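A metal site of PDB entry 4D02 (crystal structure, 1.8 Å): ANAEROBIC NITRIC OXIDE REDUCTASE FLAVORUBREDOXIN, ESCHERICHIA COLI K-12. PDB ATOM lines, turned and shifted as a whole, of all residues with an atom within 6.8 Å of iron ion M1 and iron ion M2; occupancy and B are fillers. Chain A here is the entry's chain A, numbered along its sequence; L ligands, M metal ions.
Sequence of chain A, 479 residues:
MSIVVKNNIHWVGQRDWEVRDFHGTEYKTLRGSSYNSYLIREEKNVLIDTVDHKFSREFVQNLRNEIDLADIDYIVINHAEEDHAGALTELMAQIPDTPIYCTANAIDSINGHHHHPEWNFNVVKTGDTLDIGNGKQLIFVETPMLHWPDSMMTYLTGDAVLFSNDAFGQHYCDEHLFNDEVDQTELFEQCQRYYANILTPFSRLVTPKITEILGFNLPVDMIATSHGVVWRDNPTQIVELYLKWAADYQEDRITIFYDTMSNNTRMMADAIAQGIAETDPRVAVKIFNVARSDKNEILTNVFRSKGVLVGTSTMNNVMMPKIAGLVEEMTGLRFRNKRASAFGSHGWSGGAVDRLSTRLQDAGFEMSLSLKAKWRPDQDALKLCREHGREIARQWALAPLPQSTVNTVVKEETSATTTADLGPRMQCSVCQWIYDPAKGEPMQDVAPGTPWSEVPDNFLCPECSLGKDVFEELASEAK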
ATOM      1  N   PHE A  22      -6.443 -26.685 -30.117  1.00  0.00           N
ATOM      2  CA  PHE A  22      -5.173 -26.137 -29.681  1.00  0.00           C
ATOM      3  C   PHE A  22      -4.258 -27.290 -29.319  1.00  0.00           C
ATOM      4  O   PHE A  22      -4.741 -28.325 -28.845  1.00  0.00           O
ATOM      5  CB  PHE A  22      -5.367 -25.223 -28.465  1.00  0.00           C
ATOM      6  CG  PHE A  22      -5.171 -23.767 -28.756  1.00  0.00           C
ATOM      7  CD1 PHE A  22      -6.156 -23.047 -29.410  1.00  0.00           C
ATOM      8  CD2 PHE A  22      -4.011 -23.124 -28.353  1.00  0.00           C
ATOM      9  CE1 PHE A  22      -5.981 -21.690 -29.673  1.00  0.00           C
ATOM     10  CE2 PHE A  22      -3.831 -21.775 -28.620  1.00  0.00           C
ATOM     11  CZ  PHE A  22      -4.822 -21.053 -29.283  1.00  0.00           C
ATOM     12  N   HIS A  23      -2.957 -27.115 -29.517  1.00  0.00           N
ATOM     13  CA  HIS A  23      -1.987 -28.157 -29.213  1.00  0.00           C
ATOM     14  C   HIS A  23      -2.359 -29.469 -29.895  1.00  0.00           C
ATOM     15  O   HIS A  23      -2.561 -30.482 -29.232  1.00  0.00           O
ATOM     16  CB  HIS A  23      -1.881 -28.367 -27.697  1.00  0.00           C
ATOM     17  CG  HIS A  23      -1.381 -27.180 -26.948  1.00  0.00           C
ATOM     18  ND1 HIS A  23      -1.600 -26.999 -25.599  1.00  0.00           N
ATOM     19  CD2 HIS A  23      -0.663 -26.109 -27.358  1.00  0.00           C
ATOM     20  CE1 HIS A  23      -1.041 -25.869 -25.210  1.00  0.00           C
ATOM     21  NE2 HIS A  23      -0.471 -25.306 -26.254  1.00  0.00           N
ATOM     22  N   TYR A  35      -5.666 -13.715 -29.523  1.00  0.00           N
ATOM     23  CA  TYR A  35      -4.234 -13.534 -29.321  1.00  0.00           C
ATOM     24  C   TYR A  35      -3.985 -12.056 -29.098  1.00  0.00           C
ATOM     25  O   TYR A  35      -4.083 -11.246 -30.020  1.00  0.00           O
ATOM     26  CB  TYR A  35      -3.446 -14.075 -30.525  1.00  0.00           C
ATOM     27  CG  TYR A  35      -4.049 -15.362 -31.016  1.00  0.00           C
ATOM     28  CD1 TYR A  35      -3.879 -16.553 -30.325  1.00  0.00           C
ATOM     29  CD2 TYR A  35      -4.825 -15.380 -32.167  1.00  0.00           C
ATOM     30  CE1 TYR A  35      -4.473 -17.729 -30.755  1.00  0.00           C
ATOM     31  CE2 TYR A  35      -5.412 -16.556 -32.612  1.00  0.00           C
ATOM     32  CZ  TYR A  35      -5.241 -17.726 -31.909  1.00  0.00           C
ATOM     33  OH  TYR A  35      -5.831 -18.887 -32.363  1.00  0.00           O
ATOM     34  N   HIS A  79       7.087 -14.856 -24.633  1.00  0.00           N
ATOM     35  CA  HIS A  79       6.845 -16.295 -24.764  1.00  0.00           C
ATOM     36  C   HIS A  79       6.783 -16.592 -26.250  1.00  0.00           C
ATOM     37  O   HIS A  79       6.100 -15.899 -26.986  1.00  0.00           O
ATOM     38  CB  HIS A  79       5.548 -16.636 -24.017  1.00  0.00           C
ATOM     39  CG  HIS A  79       5.071 -18.049 -24.174  1.00  0.00           C
ATOM     40  ND1 HIS A  79       5.902 -19.139 -24.036  1.00  0.00           N
ATOM     41  CD2 HIS A  79       3.826 -18.535 -24.401  1.00  0.00           C
ATOM     42  CE1 HIS A  79       5.194 -20.244 -24.188  1.00  0.00           C
ATOM     43  NE2 HIS A  79       3.933 -19.905 -24.414  1.00  0.00           N
ATOM     44  N   GLU A  81       5.903 -19.370 -28.079  1.00  0.00           N
ATOM     45  CA  GLU A  81       4.989 -20.331 -28.691  1.00  0.00           C
ATOM     46  C   GLU A  81       4.302 -19.694 -29.912  1.00  0.00           C
ATOM     47  O   GLU A  81       4.088 -18.484 -29.954  1.00  0.00           O
ATOM     48  CB  GLU A  81       3.957 -20.821 -27.679  1.00  0.00           C
ATOM     49  CG  GLU A  81       3.209 -22.063 -28.129  1.00  0.00           C
ATOM     50  CD  GLU A  81       2.556 -22.807 -26.983  1.00  0.00           C
ATOM     51  OE1 GLU A  81       2.531 -22.279 -25.845  1.00  0.00           O
ATOM     52  OE2 GLU A  81       2.080 -23.941 -27.212  1.00  0.00           O
ATOM     53  N   ASP A  83       1.492 -19.335 -31.077  1.00  0.00           N
ATOM     54  CA  ASP A  83       0.272 -18.555 -30.993  1.00  0.00           C
ATOM     55  C   ASP A  83       0.552 -17.122 -30.526  1.00  0.00           C
ATOM     56  O   ASP A  83      -0.351 -16.295 -30.492  1.00  0.00           O
ATOM     57  CB  ASP A  83      -0.756 -19.242 -30.067  1.00  0.00           C
ATOM     58  CG  ASP A  83      -0.230 -19.490 -28.655  1.00  0.00           C
ATOM     59  OD1 ASP A  83       0.984 -19.751 -28.489  1.00  0.00           O
ATOM     60  OD2 ASP A  83      -1.042 -19.428 -27.715  1.00  0.00           O
ATOM     61  N   HIS A  84       1.805 -16.832 -30.192  1.00  0.00           N
ATOM     62  CA  HIS A  84       2.179 -15.468 -29.795  1.00  0.00           C
ATOM     63  C   HIS A  84       3.343 -14.901 -30.600  1.00  0.00           C
ATOM     64  O   HIS A  84       3.325 -13.726 -30.952  1.00  0.00           O
ATOM     65  CB  HIS A  84       2.494 -15.424 -28.311  1.00  0.00           C
ATOM     66  CG  HIS A  84       1.357 -15.909 -27.469  1.00  0.00           C
ATOM     67  ND1 HIS A  84       0.132 -15.283 -27.463  1.00  0.00           N
ATOM     68  CD2 HIS A  84       1.234 -16.989 -26.661  1.00  0.00           C
ATOM     69  CE1 HIS A  84      -0.688 -15.946 -26.677  1.00  0.00           C
ATOM     70  NE2 HIS A  84      -0.046 -16.983 -26.174  1.00  0.00           N
ATOM     71  N   HIS A 147       4.353 -21.066 -18.882  1.00  0.00           N
ATOM     72  CA  HIS A 147       4.415 -22.528 -18.807  1.00  0.00           C
ATOM     73  C   HIS A 147       5.572 -23.138 -19.615  1.00  0.00           C
ATOM     74  O   HIS A 147       5.709 -24.360 -19.692  1.00  0.00           O
ATOM     75  CB  HIS A 147       3.088 -23.120 -19.295  1.00  0.00           C
ATOM     76  CG  HIS A 147       2.800 -22.840 -20.736  1.00  0.00           C
ATOM     77  ND1 HIS A 147       2.807 -23.833 -21.702  1.00  0.00           N
ATOM     78  CD2 HIS A 147       2.523 -21.685 -21.380  1.00  0.00           C
ATOM     79  CE1 HIS A 147       2.538 -23.293 -22.881  1.00  0.00           C
ATOM     80  NE2 HIS A 147       2.363 -22.001 -22.708  1.00  0.00           N
ATOM     81  N   TRP A 148       6.397 -22.289 -20.229  1.00  0.00           N
ATOM     82  CA  TRP A 148       7.561 -22.746 -20.984  1.00  0.00           C
ATOM     83  C   TRP A 148       8.844 -22.226 -20.338  1.00  0.00           C
ATOM     84  O   TRP A 148       8.789 -21.266 -19.566  1.00  0.00           O
ATOM     85  CB  TRP A 148       7.506 -22.271 -22.439  1.00  0.00           C
ATOM     86  CG  TRP A 148       6.805 -23.203 -23.378  1.00  0.00           C
ATOM     87  CD1 TRP A 148       6.014 -24.273 -23.053  1.00  0.00           C
ATOM     88  CD2 TRP A 148       6.827 -23.125 -24.814  1.00  0.00           C
ATOM     89  NE1 TRP A 148       5.552 -24.876 -24.208  1.00  0.00           N
ATOM     90  CE2 TRP A 148       6.031 -24.198 -25.294  1.00  0.00           C
ATOM     91  CE3 TRP A 148       7.442 -22.278 -25.736  1.00  0.00           C
ATOM     92  CZ2 TRP A 148       5.841 -24.432 -26.668  1.00  0.00           C
ATOM     93  CZ3 TRP A 148       7.252 -22.505 -27.097  1.00  0.00           C
ATOM     94  CH2 TRP A 148       6.458 -23.580 -27.544  1.00  0.00           C
ATOM     95  N   SER A 151       9.232 -18.367 -20.801  1.00  0.00           N
ATOM     96  CA  SER A 151       8.158 -17.475 -20.376  1.00  0.00           C
ATOM     97  C   SER A 151       8.598 -16.367 -19.425  1.00  0.00           C
ATOM     98  O   SER A 151       9.369 -16.583 -18.485  1.00  0.00           O
ATOM     99  CB  SER A 151       7.036 -18.274 -19.716  1.00  0.00           C
ATOM    100  OG  SER A 151       6.527 -19.272 -20.585  1.00  0.00           O
ATOM    101  N   ASN A 165       1.180 -12.472 -20.435  1.00  0.00           N
ATOM    102  CA  ASN A 165       1.148 -13.487 -21.496  1.00  0.00           C
ATOM    103  C   ASN A 165       0.126 -14.562 -21.133  1.00  0.00           C
ATOM    104  O   ASN A 165      -0.993 -14.224 -20.770  1.00  0.00           O
ATOM    105  CB  ASN A 165       2.539 -14.069 -21.743  1.00  0.00           C
ATOM    106  CG  ASN A 165       2.631 -14.852 -23.053  1.00  0.00           C
ATOM    107  OD1 ASN A 165       2.551 -16.080 -23.065  1.00  0.00           O
ATOM    108  ND2 ASN A 165       2.787 -14.149 -24.162  1.00  0.00           N
ATOM    109  N   ASP A 166       0.492 -15.843 -21.229  1.00  0.00           N
ATOM    110  CA  ASP A 166      -0.466 -16.932 -21.007  1.00  0.00           C
ATOM    111  C   ASP A 166      -1.110 -16.919 -19.613  1.00  0.00           C
ATOM    112  O   ASP A 166      -2.283 -17.266 -19.445  1.00  0.00           O
ATOM    113  CB  ASP A 166       0.202 -18.304 -21.225  1.00  0.00           C
ATOM    114  CG  ASP A 166       0.346 -18.696 -22.697  1.00  0.00           C
ATOM    115  OD1 ASP A 166      -0.476 -18.280 -23.547  1.00  0.00           O
ATOM    116  OD2 ASP A 166       1.302 -19.449 -22.986  1.00  0.00           O
ATOM    117  N   HIS A 171      -9.026 -19.119 -23.066  1.00  0.00           N
ATOM    118  CA  HIS A 171      -9.484 -19.168 -24.458  1.00  0.00           C
ATOM    119  C   HIS A 171     -10.970 -18.889 -24.502  1.00  0.00           C
ATOM    120  O   HIS A 171     -11.794 -19.750 -24.213  1.00  0.00           O
ATOM    121  CB  HIS A 171      -9.155 -20.522 -25.081  1.00  0.00           C
ATOM    122  CG  HIS A 171      -7.686 -20.819 -25.109  1.00  0.00           C
ATOM    123  ND1 HIS A 171      -6.785 -20.010 -25.769  1.00  0.00           N
ATOM    124  CD2 HIS A 171      -6.958 -21.808 -24.548  1.00  0.00           C
ATOM    125  CE1 HIS A 171      -5.569 -20.491 -25.621  1.00  0.00           C
ATOM    126  NE2 HIS A 171      -5.646 -21.593 -24.887  1.00  0.00           N
ATOM    127  N   TYR A 194      -8.824 -23.837 -18.725  1.00  0.00           N
ATOM    128  CA  TYR A 194      -7.474 -23.455 -19.073  1.00  0.00           C
ATOM    129  C   TYR A 194      -6.464 -23.871 -17.995  1.00  0.00           C
ATOM    130  O   TYR A 194      -5.473 -24.556 -18.288  1.00  0.00           O
ATOM    131  CB  TYR A 194      -7.469 -21.959 -19.276  1.00  0.00           C
ATOM    132  CG  TYR A 194      -6.207 -21.345 -19.787  1.00  0.00           C
ATOM    133  CD1 TYR A 194      -5.241 -20.872 -18.906  1.00  0.00           C
ATOM    134  CD2 TYR A 194      -6.015 -21.162 -21.151  1.00  0.00           C
ATOM    135  CE1 TYR A 194      -4.095 -20.272 -19.375  1.00  0.00           C
ATOM    136  CE2 TYR A 194      -4.874 -20.561 -21.628  1.00  0.00           C
ATOM    137  CZ  TYR A 194      -3.923 -20.115 -20.742  1.00  0.00           C
ATOM    138  OH  TYR A 194      -2.782 -19.515 -21.220  1.00  0.00           O
ATOM    139  N   ILE A 198      -3.831 -27.039 -18.727  1.00  0.00           N
ATOM    140  CA  ILE A 198      -2.520 -26.587 -19.163  1.00  0.00           C
ATOM    141  C   ILE A 198      -1.566 -26.342 -17.982  1.00  0.00           C
ATOM    142  O   ILE A 198      -0.379 -26.701 -18.038  1.00  0.00           O
ATOM    143  CB  ILE A 198      -2.609 -25.284 -20.008  1.00  0.00           C
ATOM    144  CG1 ILE A 198      -3.625 -25.441 -21.136  1.00  0.00           C
ATOM    145  CG2 ILE A 198      -1.239 -24.911 -20.575  1.00  0.00           C
ATOM    146  CD1 ILE A 198      -3.209 -26.427 -22.173  1.00  0.00           C
ATOM    147  N   SER A 226      -2.294 -12.630 -22.747  1.00  0.00           N
ATOM    148  CA  SER A 226      -2.137 -12.875 -24.170  1.00  0.00           C
ATOM    149  C   SER A 226      -3.331 -13.616 -24.779  1.00  0.00           C
ATOM    150  O   SER A 226      -3.368 -13.859 -25.987  1.00  0.00           O
ATOM    151  CB  SER A 226      -0.848 -13.641 -24.419  1.00  0.00           C
ATOM    152  OG  SER A 226      -0.904 -14.911 -23.801  1.00  0.00           O
ATOM    153  N   HIS A 227      -4.291 -13.986 -23.926  1.00  0.00           N
ATOM    154  CA  HIS A 227      -5.497 -14.681 -24.375  1.00  0.00           C
ATOM    155  C   HIS A 227      -6.717 -14.156 -23.653  1.00  0.00           C
ATOM    156  O   HIS A 227      -6.761 -14.176 -22.419  1.00  0.00           O
ATOM    157  CB  HIS A 227      -5.415 -16.193 -24.119  1.00  0.00           C
ATOM    158  CG  HIS A 227      -4.397 -16.905 -24.960  1.00  0.00           C
ATOM    159  ND1 HIS A 227      -4.532 -17.080 -26.314  1.00  0.00           N
ATOM    160  CD2 HIS A 227      -3.241 -17.523 -24.603  1.00  0.00           C
ATOM    161  CE1 HIS A 227      -3.495 -17.756 -26.771  1.00  0.00           C
ATOM    162  NE2 HIS A 227      -2.695 -18.041 -25.760  1.00  0.00           N
HETATM  163  O1  LIG L   1       1.122 -19.758 -25.858  1.00  0.00           O
HETATM  164  P1  LG2 L   2      -1.283 -21.887 -24.879  1.00  0.00           P
HETATM  165  O1  LG2 L   2      -1.233 -22.286 -26.344  1.00  0.00           O
HETATM  166  O2  LG2 L   2       0.059 -22.166 -24.246  1.00  0.00           O
HETATM  167  O3  LG2 L   2      -1.592 -20.420 -24.743  1.00  0.00           O
HETATM  168  O4  LG2 L   2      -2.356 -22.671 -24.177  1.00  0.00           O
HETATM  169  N1  LG3 L   3       9.224 -29.984 -24.408  1.00  0.00           N
HETATM  170  C1  LG3 L   3      10.040 -30.718 -23.578  1.00  0.00           C
HETATM  171  O1  LG3 L   3      11.231 -30.865 -23.863  1.00  0.00           O
HETATM  172  N2  LG3 L   3       9.529 -31.282 -22.418  1.00  0.00           N
HETATM  173  C2  LG3 L   3       8.206 -31.127 -22.080  1.00  0.00           C
HETATM  174  O2  LG3 L   3       7.785 -31.645 -21.038  1.00  0.00           O
HETATM  175  C3  LG3 L   3       7.361 -30.398 -22.917  1.00  0.00           C
HETATM  176  N3  LG3 L   3       6.025 -30.212 -22.604  1.00  0.00           N
HETATM  177  C4  LG3 L   3       5.205 -29.484 -23.455  1.00  0.00           C
HETATM  178  C5  LG3 L   3       3.858 -29.311 -23.159  1.00  0.00           C
HETATM  179  C6  LG3 L   3       3.038 -28.583 -24.010  1.00  0.00           C
HETATM  180  C7  LG3 L   3       1.580 -28.375 -23.684  1.00  0.00           C
HETATM  181  C8  LG3 L   3       3.572 -28.007 -25.159  1.00  0.00           C
HETATM  182  C9  LG3 L   3       2.683 -27.201 -26.080  1.00  0.00           C
HETATM  183  C10 LG3 L   3       4.914 -28.179 -25.463  1.00  0.00           C
HETATM  184  C11 LG3 L   3       5.740 -28.915 -24.616  1.00  0.00           C
HETATM  185  N4  LG3 L   3       7.075 -29.094 -24.917  1.00  0.00           N
HETATM  186  C12 LG3 L   3       7.889 -29.835 -24.075  1.00  0.00           C
HETATM  187  C13 LG3 L   3       7.683 -28.499 -26.152  1.00  0.00           C
HETATM  188  C14 LG3 L   3       7.370 -29.360 -27.376  1.00  0.00           C
HETATM  189  O3  LG3 L   3       7.860 -30.680 -27.212  1.00  0.00           O
HETATM  190  C15 LG3 L   3       8.000 -28.669 -28.583  1.00  0.00           C
HETATM  191  O4  LG3 L   3       7.211 -27.528 -28.867  1.00  0.00           O
HETATM  192  C16 LG3 L   3       8.082 -29.596 -29.782  1.00  0.00           C
HETATM  193  O5  LG3 L   3       8.902 -29.026 -30.760  1.00  0.00           O
HETATM  194  C17 LG3 L   3       6.691 -29.776 -30.353  1.00  0.00           C
HETATM  195  O6  LG3 L   3       6.716 -30.754 -31.374  1.00  0.00           O
HETATM  196  P1  LG3 L   3       5.342 -30.993 -32.179  1.00  0.00           P
HETATM  197  O7  LG3 L   3       5.501 -32.168 -33.118  1.00  0.00           O
HETATM  198  O8  LG3 L   3       4.228 -31.235 -31.193  1.00  0.00           O
HETATM  199  O9  LG3 L   3       5.053 -29.733 -32.969  1.00  0.00           O
HETATM  200 FE    FE M   1       1.917 -20.858 -24.387  1.00  0.00          FE
HETATM  201 FE    FE M   2      -0.727 -18.902 -25.526  1.00  0.00          FE
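The side-chain carboxylate of Glu 81 lies within hydrogen-bond range of a ring nitrogen (NE2) of His 23, 3.0 Å away.
A ring nitrogen (NE2) of His 84 sits close to the side-chain hydroxyl (OG) of Ser 226 (3.3 Å).
N of His 147 is in hydrogen-bond range of OG of Ser 151, at 3.3 Å.
The side-chain hydroxyl of Ser 226 sits at hydrogen-bond distance from the backbone NH of Asp 166, 3.1 Å away.
OH of Tyr 194 sits at hydrogen-bond distance from O of Asp 166, at 2.9 Å.
An oxygen (O3) of LG2 L2 binds iron ion M2.
An oxygen (O1) of LIG L1 is bound to iron ion M2.
OD1 of Asp 166 is bound to iron ion M2 (2.1 Å).
Iron ion M2 is bound by NE2 of His 84 (2.1 Å).
NE2 of His 227 is bound to iron ion M2, at 2.2 Å.
OD2 of Asp 83 binds iron ion M2, at 2.3 Å.
Iron ion M1 is bound by O1 of LIG L1, 2.0 Å away.
NE2 of His 147 binds iron ion M1 (2.1 Å).
The side-chain carboxylate (OD2) of Asp 166 is bound to iron ion M1.
OE1 of Glu 81 binds iron ion M1 (2.1 Å).
A ring nitrogen (NE2) of His 79 binds iron ion M1 (2.2 Å).
Iron ion M1 is bound by O2 of LG2 L2 (2.3 Å).
Within 4 Å of iron ion M1: His 79, Glu 81, His 147 and Asp 166.
The nearest printed residue that does not touch iron ion M1 is Asp 83 (4.3 Å).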
